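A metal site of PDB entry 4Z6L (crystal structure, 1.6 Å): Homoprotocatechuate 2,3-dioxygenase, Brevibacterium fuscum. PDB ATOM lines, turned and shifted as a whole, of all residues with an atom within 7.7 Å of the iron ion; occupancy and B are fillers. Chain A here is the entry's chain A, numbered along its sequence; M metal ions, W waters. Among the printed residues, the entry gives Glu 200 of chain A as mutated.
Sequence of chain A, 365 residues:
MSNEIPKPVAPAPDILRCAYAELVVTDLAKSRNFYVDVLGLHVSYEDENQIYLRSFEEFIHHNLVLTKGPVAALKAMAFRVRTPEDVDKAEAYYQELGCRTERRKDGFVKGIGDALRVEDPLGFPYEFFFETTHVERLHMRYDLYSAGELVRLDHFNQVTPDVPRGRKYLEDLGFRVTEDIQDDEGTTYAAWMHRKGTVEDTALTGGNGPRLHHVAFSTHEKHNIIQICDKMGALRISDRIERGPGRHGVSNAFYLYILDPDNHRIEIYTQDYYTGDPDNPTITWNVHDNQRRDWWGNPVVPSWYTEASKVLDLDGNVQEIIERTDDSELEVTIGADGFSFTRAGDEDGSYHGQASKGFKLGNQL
Water W3 bridges the side-chain carboxylate (OE2) of Glu 200 (2.6 Å) and the side-chain carboxylate (OE2) of Glu 267 (3.3 Å). Water W2 lies within hydrogen-bond range of the side-chain carboxylate (OE1) of Glu 200 (2.5 Å), the side-chain amide nitrogen (ND2) of Asn 157 (2.9 Å) and the indole nitrogen (NE1) of Trp 192 (3.3 Å).
The iron ion is bound by water W1, OE1 of Glu 267, water W2, water W3, NE2 of His 214 and NE2 of His 155.
Glu 200 touches the iron ion. Within 4 Å of the iron ion: His 155, Glu 200, His 214 and Glu 267.
OH of Tyr 257 is in hydrogen-bond range of OE2 of Glu 267 (3.2 Å). A ring nitrogen (ND1) of His 155 is in hydrogen-bond range of the side-chain carboxylate (OD2) of Asp 154 (2.7 Å). The indole nitrogen (NE1) of Trp 192 lies close to the side-chain carboxylate (OE1) of Glu 200 (3.4 Å). A ring nitrogen (NE2) of His 248 sits at hydrogen-bond distance from the side-chain carboxylate (OE2) of Glu 267, 2.7 Å away. A ring nitrogen (NE2) of His 155 sits close to the side-chain carboxylate of Glu 200, at 3.3 Å. OE2 of Glu 200 sits at hydrogen-bond distance from OH of Tyr 269, at 3.2 Å. N of Glu 267 sits at hydrogen-bond distance from O of Val 215, at 3.0 Å. The backbone NH (N) of Asn 157 lies within hydrogen-bond range of the backbone carbonyl oxygen (O) of His 214 (3.0 Å).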
ATOM      1  N   ASP A 154      -3.059  10.194 -21.310  1.00  0.00           N
ATOM      2  CA  ASP A 154      -4.307  10.657 -20.710  1.00  0.00           C
ATOM      3  C   ASP A 154      -5.418   9.595 -20.715  1.00  0.00           C
ATOM      4  O   ASP A 154      -6.097   9.396 -19.680  1.00  0.00           O
ATOM      5  CB  ASP A 154      -4.843  11.936 -21.308  1.00  0.00           C
ATOM      6  CG  ASP A 154      -6.035  12.462 -20.470  1.00  0.00           C
ATOM      7  OD1 ASP A 154      -5.779  12.935 -19.306  1.00  0.00           O
ATOM      8  OD2 ASP A 154      -7.209  12.326 -20.942  1.00  0.00           O
ATOM      9  N   HIS A 155      -5.652   8.965 -21.866  1.00  0.00           N
ATOM     10  CA  HIS A 155      -6.796   8.034 -22.001  1.00  0.00           C
ATOM     11  C   HIS A 155      -6.743   7.157 -23.206  1.00  0.00           C
ATOM     12  O   HIS A 155      -5.964   7.396 -24.116  1.00  0.00           O
ATOM     13  CB  HIS A 155      -8.137   8.818 -22.007  1.00  0.00           C
ATOM     14  CG  HIS A 155      -8.325   9.709 -23.195  1.00  0.00           C
ATOM     15  ND1 HIS A 155      -8.017  11.058 -23.193  1.00  0.00           N
ATOM     16  CD2 HIS A 155      -8.856   9.452 -24.428  1.00  0.00           C
ATOM     17  CE1 HIS A 155      -8.343  11.580 -24.363  1.00  0.00           C
ATOM     18  NE2 HIS A 155      -8.842  10.621 -25.125  1.00  0.00           N
ATOM     19  N   PHE A 156      -7.614   6.155 -23.230  1.00  0.00           N
ATOM     20  CA  PHE A 156      -7.915   5.369 -24.425  1.00  0.00           C
ATOM     21  C   PHE A 156      -9.347   5.699 -24.891  1.00  0.00           C
ATOM     22  O   PHE A 156     -10.157   6.226 -24.094  1.00  0.00           O
ATOM     23  CB  PHE A 156      -7.918   3.867 -24.082  1.00  0.00           C
ATOM     24  CG  PHE A 156      -6.714   3.389 -23.316  1.00  0.00           C
ATOM     25  CD1 PHE A 156      -5.429   3.562 -23.817  1.00  0.00           C
ATOM     26  CD2 PHE A 156      -6.866   2.741 -22.077  1.00  0.00           C
ATOM     27  CE1 PHE A 156      -4.326   3.111 -23.124  1.00  0.00           C
ATOM     28  CE2 PHE A 156      -5.751   2.299 -21.365  1.00  0.00           C
ATOM     29  CZ  PHE A 156      -4.503   2.483 -21.883  1.00  0.00           C
ATOM     30  N   ASN A 157      -9.671   5.390 -26.135  1.00  0.00           N
ATOM     31  CA  ASN A 157     -11.062   5.464 -26.617  1.00  0.00           C
ATOM     32  C   ASN A 157     -11.376   4.238 -27.484  1.00  0.00           C
ATOM     33  O   ASN A 157     -10.661   3.950 -28.437  1.00  0.00           O
ATOM     34  CB  ASN A 157     -11.291   6.774 -27.352  1.00  0.00           C
ATOM     35  CG  ASN A 157     -12.715   6.966 -27.812  1.00  0.00           C
ATOM     36  OD1 ASN A 157     -13.250   6.161 -28.570  1.00  0.00           O
ATOM     37  ND2 ASN A 157     -13.321   8.079 -27.380  1.00  0.00           N
ATOM     38  N   TRP A 192     -17.941   8.914 -21.891  1.00  0.00           N
ATOM     39  CA  TRP A 192     -16.608   9.091 -21.332  1.00  0.00           C
ATOM     40  C   TRP A 192     -16.616   8.757 -19.864  1.00  0.00           C
ATOM     41  O   TRP A 192     -17.542   9.133 -19.156  1.00  0.00           O
ATOM     42  CB  TRP A 192     -16.207  10.548 -21.516  1.00  0.00           C
ATOM     43  CG  TRP A 192     -15.879  10.939 -22.937  1.00  0.00           C
ATOM     44  CD1 TRP A 192     -14.623  11.148 -23.442  1.00  0.00           C
ATOM     45  CD2 TRP A 192     -16.788  11.212 -24.009  1.00  0.00           C
ATOM     46  NE1 TRP A 192     -14.678  11.494 -24.763  1.00  0.00           N
ATOM     47  CE2 TRP A 192     -15.986  11.533 -25.147  1.00  0.00           C
ATOM     48  CE3 TRP A 192     -18.194  11.202 -24.137  1.00  0.00           C
ATOM     49  CZ2 TRP A 192     -16.545  11.860 -26.380  1.00  0.00           C
ATOM     50  CZ3 TRP A 192     -18.742  11.475 -25.369  1.00  0.00           C
ATOM     51  CH2 TRP A 192     -17.934  11.847 -26.470  1.00  0.00           C
ATOM     52  N   GLU A 200     -11.614  11.448 -18.586  1.00  0.00           N
ATOM     53  CA  GLU A 200     -11.617  10.090 -19.085  1.00  0.00           C
ATOM     54  C   GLU A 200     -10.303   9.373 -18.750  1.00  0.00           C
ATOM     55  O   GLU A 200      -9.234   9.957 -18.805  1.00  0.00           O
ATOM     56  CB  GLU A 200     -11.867  10.066 -20.586  1.00  0.00           C
ATOM     57  CG  GLU A 200     -11.046  11.106 -21.331  1.00  0.00           C
ATOM     58  CD  GLU A 200     -11.410  11.314 -22.814  1.00  0.00           C
ATOM     59  OE1 GLU A 200     -11.699  10.305 -23.506  1.00  0.00           O
ATOM     60  OE2 GLU A 200     -11.390  12.500 -23.286  1.00  0.00           O
ATOM     61  N   ALA A 203     -13.038   5.586 -22.869  1.00  0.00           N
ATOM     62  CA  ALA A 203     -14.201   6.217 -23.440  1.00  0.00           C
ATOM     63  C   ALA A 203     -14.752   5.276 -24.481  1.00  0.00           C
ATOM     64  O   ALA A 203     -14.004   4.456 -25.056  1.00  0.00           O
ATOM     65  CB  ALA A 203     -13.840   7.579 -24.031  1.00  0.00           C
ATOM     66  N   THR A 205     -16.979   4.901 -28.027  1.00  0.00           N
ATOM     67  CA  THR A 205     -17.498   5.495 -29.252  1.00  0.00           C
ATOM     68  C   THR A 205     -18.360   4.433 -29.925  1.00  0.00           C
ATOM     69  O   THR A 205     -17.919   3.308 -30.148  1.00  0.00           O
ATOM     70  CB  THR A 205     -16.388   5.960 -30.192  1.00  0.00           C
ATOM     71  OG1 THR A 205     -15.567   6.919 -29.521  1.00  0.00           O
ATOM     72  CG2 THR A 205     -16.938   6.544 -31.464  1.00  0.00           C
ATOM     73  N   HIS A 213     -10.265   3.201 -30.964  1.00  0.00           N
ATOM     74  CA  HIS A 213     -10.341   4.444 -31.653  1.00  0.00           C
ATOM     75  C   HIS A 213      -9.051   5.261 -31.596  1.00  0.00           C
ATOM     76  O   HIS A 213      -8.578   5.681 -32.622  1.00  0.00           O
ATOM     77  CB  HIS A 213     -11.525   5.293 -31.141  1.00  0.00           C
ATOM     78  CG  HIS A 213     -11.891   6.331 -32.119  1.00  0.00           C
ATOM     79  ND1 HIS A 213     -11.235   7.535 -32.177  1.00  0.00           N
ATOM     80  CD2 HIS A 213     -12.788   6.348 -33.147  1.00  0.00           C
ATOM     81  CE1 HIS A 213     -11.722   8.269 -33.158  1.00  0.00           C
ATOM     82  NE2 HIS A 213     -12.673   7.572 -33.768  1.00  0.00           N
ATOM     83  N   HIS A 214      -8.536   5.496 -30.401  1.00  0.00           N
ATOM     84  CA  HIS A 214      -7.264   6.175 -30.277  1.00  0.00           C
ATOM     85  C   HIS A 214      -6.677   5.983 -28.894  1.00  0.00           C
ATOM     86  O   HIS A 214      -7.341   5.520 -27.976  1.00  0.00           O
ATOM     87  CB  HIS A 214      -7.429   7.662 -30.618  1.00  0.00           C
ATOM     88  CG  HIS A 214      -8.383   8.396 -29.720  1.00  0.00           C
ATOM     89  ND1 HIS A 214      -9.686   8.644 -30.074  1.00  0.00           N
ATOM     90  CD2 HIS A 214      -8.202   9.013 -28.534  1.00  0.00           C
ATOM     91  CE1 HIS A 214     -10.275   9.354 -29.142  1.00  0.00           C
ATOM     92  NE2 HIS A 214      -9.394   9.604 -28.200  1.00  0.00           N
ATOM     93  N   VAL A 215      -5.400   6.367 -28.802  1.00  0.00           N
ATOM     94  CA  VAL A 215      -4.703   6.558 -27.553  1.00  0.00           C
ATOM     95  C   VAL A 215      -4.391   8.052 -27.449  1.00  0.00           C
ATOM     96  O   VAL A 215      -4.020   8.661 -28.429  1.00  0.00           O
ATOM     97  CB  VAL A 215      -3.392   5.724 -27.545  1.00  0.00           C
ATOM     98  CG1 VAL A 215      -2.642   5.974 -26.265  1.00  0.00           C
ATOM     99  CG2 VAL A 215      -3.719   4.231 -27.709  1.00  0.00           C
ATOM    100  N   ALA A 216      -4.565   8.646 -26.260  1.00  0.00           N
ATOM    101  CA  ALA A 216      -4.392  10.094 -26.138  1.00  0.00           C
ATOM    102  C   ALA A 216      -3.253  10.450 -25.200  1.00  0.00           C
ATOM    103  O   ALA A 216      -3.149   9.897 -24.096  1.00  0.00           O
ATOM    104  CB  ALA A 216      -5.689  10.709 -25.630  1.00  0.00           C
ATOM    105  N   HIS A 248     -12.576  20.751 -27.918  1.00  0.00           N
ATOM    106  CA  HIS A 248     -13.682  19.814 -27.807  1.00  0.00           C
ATOM    107  C   HIS A 248     -14.879  20.510 -27.120  1.00  0.00           C
ATOM    108  O   HIS A 248     -14.691  21.367 -26.242  1.00  0.00           O
ATOM    109  CB  HIS A 248     -13.326  18.610 -26.954  1.00  0.00           C
ATOM    110  CG  HIS A 248     -12.550  17.557 -27.662  1.00  0.00           C
ATOM    111  ND1 HIS A 248     -12.962  16.983 -28.848  1.00  0.00           N
ATOM    112  CD2 HIS A 248     -11.404  16.910 -27.308  1.00  0.00           C
ATOM    113  CE1 HIS A 248     -12.090  16.066 -29.216  1.00  0.00           C
ATOM    114  NE2 HIS A 248     -11.142  15.988 -28.304  1.00  0.00           N
ATOM    115  N   VAL A 250     -17.453  18.119 -25.636  1.00  0.00           N
ATOM    116  CA  VAL A 250     -17.262  17.073 -24.666  1.00  0.00           C
ATOM    117  C   VAL A 250     -15.787  17.100 -24.182  1.00  0.00           C
ATOM    118  O   VAL A 250     -14.891  16.978 -24.986  1.00  0.00           O
ATOM    119  CB  VAL A 250     -17.522  15.695 -25.269  1.00  0.00           C
ATOM    120  CG1 VAL A 250     -17.137  14.629 -24.254  1.00  0.00           C
ATOM    121  CG2 VAL A 250     -18.984  15.539 -25.638  1.00  0.00           C
ATOM    122  N   SER A 251     -15.595  17.282 -22.886  1.00  0.00           N
ATOM    123  CA  SER A 251     -14.257  17.336 -22.213  1.00  0.00           C
ATOM    124  C   SER A 251     -13.686  18.728 -22.084  1.00  0.00           C
ATOM    125  O   SER A 251     -12.821  18.968 -21.242  1.00  0.00           O
ATOM    126  CB  SER A 251     -13.195  16.407 -22.806  1.00  0.00           C
ATOM    127  OG  SER A 251     -12.555  17.004 -23.931  1.00  0.00           O
ATOM    128  N   TYR A 255      -7.442  19.879 -28.601  1.00  0.00           N
ATOM    129  CA  TYR A 255      -7.150  18.566 -29.168  1.00  0.00           C
ATOM    130  C   TYR A 255      -6.622  18.593 -30.574  1.00  0.00           C
ATOM    131  O   TYR A 255      -6.744  19.605 -31.290  1.00  0.00           O
ATOM    132  CB  TYR A 255      -8.399  17.674 -29.179  1.00  0.00           C
ATOM    133  CG  TYR A 255      -9.398  18.074 -30.253  1.00  0.00           C
ATOM    134  CD1 TYR A 255      -9.345  17.535 -31.530  1.00  0.00           C
ATOM    135  CD2 TYR A 255     -10.430  18.974 -29.970  1.00  0.00           C
ATOM    136  CE1 TYR A 255     -10.280  17.903 -32.498  1.00  0.00           C
ATOM    137  CE2 TYR A 255     -11.363  19.350 -30.934  1.00  0.00           C
ATOM    138  CZ  TYR A 255     -11.284  18.800 -32.187  1.00  0.00           C
ATOM    139  OH  TYR A 255     -12.168  19.167 -33.141  1.00  0.00           O
ATOM    140  N   TYR A 257      -5.992  15.179 -33.691  1.00  0.00           N
ATOM    141  CA  TYR A 257      -5.931  13.740 -34.061  1.00  0.00           C
ATOM    142  C   TYR A 257      -5.008  13.559 -35.270  1.00  0.00           C
ATOM    143  O   TYR A 257      -5.185  14.187 -36.315  1.00  0.00           O
ATOM    144  CB  TYR A 257      -7.303  13.204 -34.466  1.00  0.00           C
ATOM    145  CG  TYR A 257      -8.305  13.245 -33.343  1.00  0.00           C
ATOM    146  CD1 TYR A 257      -8.291  12.278 -32.341  1.00  0.00           C
ATOM    147  CD2 TYR A 257      -9.242  14.256 -33.256  1.00  0.00           C
ATOM    148  CE1 TYR A 257      -9.163  12.308 -31.277  1.00  0.00           C
ATOM    149  CE2 TYR A 257     -10.144  14.293 -32.186  1.00  0.00           C
ATOM    150  CZ  TYR A 257     -10.109  13.314 -31.218  1.00  0.00           C
ATOM    151  OH  TYR A 257     -11.046  13.356 -30.201  1.00  0.00           O
ATOM    152  N   GLU A 267      -4.470  10.902 -30.297  1.00  0.00           N
ATOM    153  CA  GLU A 267      -4.926  12.225 -29.886  1.00  0.00           C
ATOM    154  C   GLU A 267      -3.870  12.924 -29.019  1.00  0.00           C
ATOM    155  O   GLU A 267      -3.266  12.299 -28.136  1.00  0.00           O
ATOM    156  CB  GLU A 267      -6.226  12.146 -29.072  1.00  0.00           C
ATOM    157  CG  GLU A 267      -6.861  13.512 -28.863  1.00  0.00           C
ATOM    158  CD  GLU A 267      -8.152  13.449 -28.084  1.00  0.00           C
ATOM    159  OE1 GLU A 267      -8.419  12.372 -27.507  1.00  0.00           O
ATOM    160  OE2 GLU A 267      -8.884  14.448 -28.036  1.00  0.00           O
ATOM    161  N   ILE A 268      -3.700  14.218 -29.263  1.00  0.00           N
ATOM    162  CA  ILE A 268      -2.985  15.094 -28.398  1.00  0.00           C
ATOM    163  C   ILE A 268      -4.003  16.013 -27.751  1.00  0.00           C
ATOM    164  O   ILE A 268      -4.887  16.527 -28.434  1.00  0.00           O
ATOM    165  CB  ILE A 268      -1.920  15.899 -29.172  1.00  0.00           C
ATOM    166  CG1 ILE A 268      -1.243  15.067 -30.283  1.00  0.00           C
ATOM    167  CG2 ILE A 268      -0.898  16.435 -28.184  1.00  0.00           C
ATOM    168  CD1 ILE A 268      -0.449  13.912 -29.829  1.00  0.00           C
ATOM    169  N   TYR A 269      -3.902  16.212 -26.451  1.00  0.00           N
ATOM    170  CA  TYR A 269      -5.005  16.689 -25.622  1.00  0.00           C
ATOM    171  C   TYR A 269      -4.451  17.594 -24.540  1.00  0.00           C
ATOM    172  O   TYR A 269      -3.369  17.348 -24.008  1.00  0.00           O
ATOM    173  CB  TYR A 269      -5.616  15.410 -25.006  1.00  0.00           C
ATOM    174  CG  TYR A 269      -6.859  15.428 -24.166  1.00  0.00           C
ATOM    175  CD1 TYR A 269      -8.118  15.270 -24.741  1.00  0.00           C
ATOM    176  CD2 TYR A 269      -6.760  15.428 -22.765  1.00  0.00           C
ATOM    177  CE1 TYR A 269      -9.247  15.206 -23.952  1.00  0.00           C
ATOM    178  CE2 TYR A 269      -7.884  15.376 -21.980  1.00  0.00           C
ATOM    179  CZ  TYR A 269      -9.125  15.255 -22.589  1.00  0.00           C
ATOM    180  OH  TYR A 269     -10.235  15.130 -21.811  1.00  0.00           O
ATOM    181  N   ARG A 293     -18.537  18.132 -30.455  1.00  0.00           N
ATOM    182  CA  ARG A 293     -17.269  17.455 -30.704  1.00  0.00           C
ATOM    183  C   ARG A 293     -16.157  18.446 -30.982  1.00  0.00           C
ATOM    184  O   ARG A 293     -15.128  18.358 -30.381  1.00  0.00           O
ATOM    185  CB  ARG A 293     -17.397  16.441 -31.831  1.00  0.00           C
ATOM    186  CG  ARG A 293     -18.179  15.196 -31.429  1.00  0.00           C
ATOM    187  CD  ARG A 293     -17.799  13.989 -32.240  1.00  0.00           C
ATOM    188  NE  ARG A 293     -18.453  12.768 -31.724  1.00  0.00           N
ATOM    189  CZ  ARG A 293     -17.983  11.950 -30.798  1.00  0.00           C
ATOM    190  NH1 ARG A 293     -16.826  12.191 -30.180  1.00  0.00           N
ATOM    191  NH2 ARG A 293     -18.679  10.871 -30.489  1.00  0.00           N
ATOM    192  N   TRP A 304     -12.988   9.884 -39.223  1.00  0.00           N
ATOM    193  CA  TRP A 304     -12.902   9.888 -37.778  1.00  0.00           C
ATOM    194  C   TRP A 304     -13.952   8.941 -37.190  1.00  0.00           C
ATOM    195  O   TRP A 304     -13.747   8.297 -36.156  1.00  0.00           O
ATOM    196  CB  TRP A 304     -13.020  11.335 -37.237  1.00  0.00           C
ATOM    197  CG  TRP A 304     -12.590  11.468 -35.806  1.00  0.00           C
ATOM    198  CD1 TRP A 304     -11.342  11.763 -35.342  1.00  0.00           C
ATOM    199  CD2 TRP A 304     -13.402  11.232 -34.666  1.00  0.00           C
ATOM    200  NE1 TRP A 304     -11.334  11.742 -33.976  1.00  0.00           N
ATOM    201  CE2 TRP A 304     -12.595  11.421 -33.546  1.00  0.00           C
ATOM    202  CE3 TRP A 304     -14.755  10.910 -34.502  1.00  0.00           C
ATOM    203  CZ2 TRP A 304     -13.074  11.271 -32.251  1.00  0.00           C
ATOM    204  CZ3 TRP A 304     -15.232  10.769 -33.201  1.00  0.00           C
ATOM    205  CH2 TRP A 304     -14.382  10.927 -32.095  1.00  0.00           C
HETATM  206 FE    FE M   1     -10.133  11.263 -26.862  1.00  0.00          FE
HETATM  207  O   HOH W   1     -11.460  12.170 -28.261  1.00  0.00           O
HETATM  208  O   HOH W   2     -11.871  10.226 -26.010  1.00  0.00           O
HETATM  209  O   HOH W   3     -10.885  13.096 -25.789  1.00  0.00           O
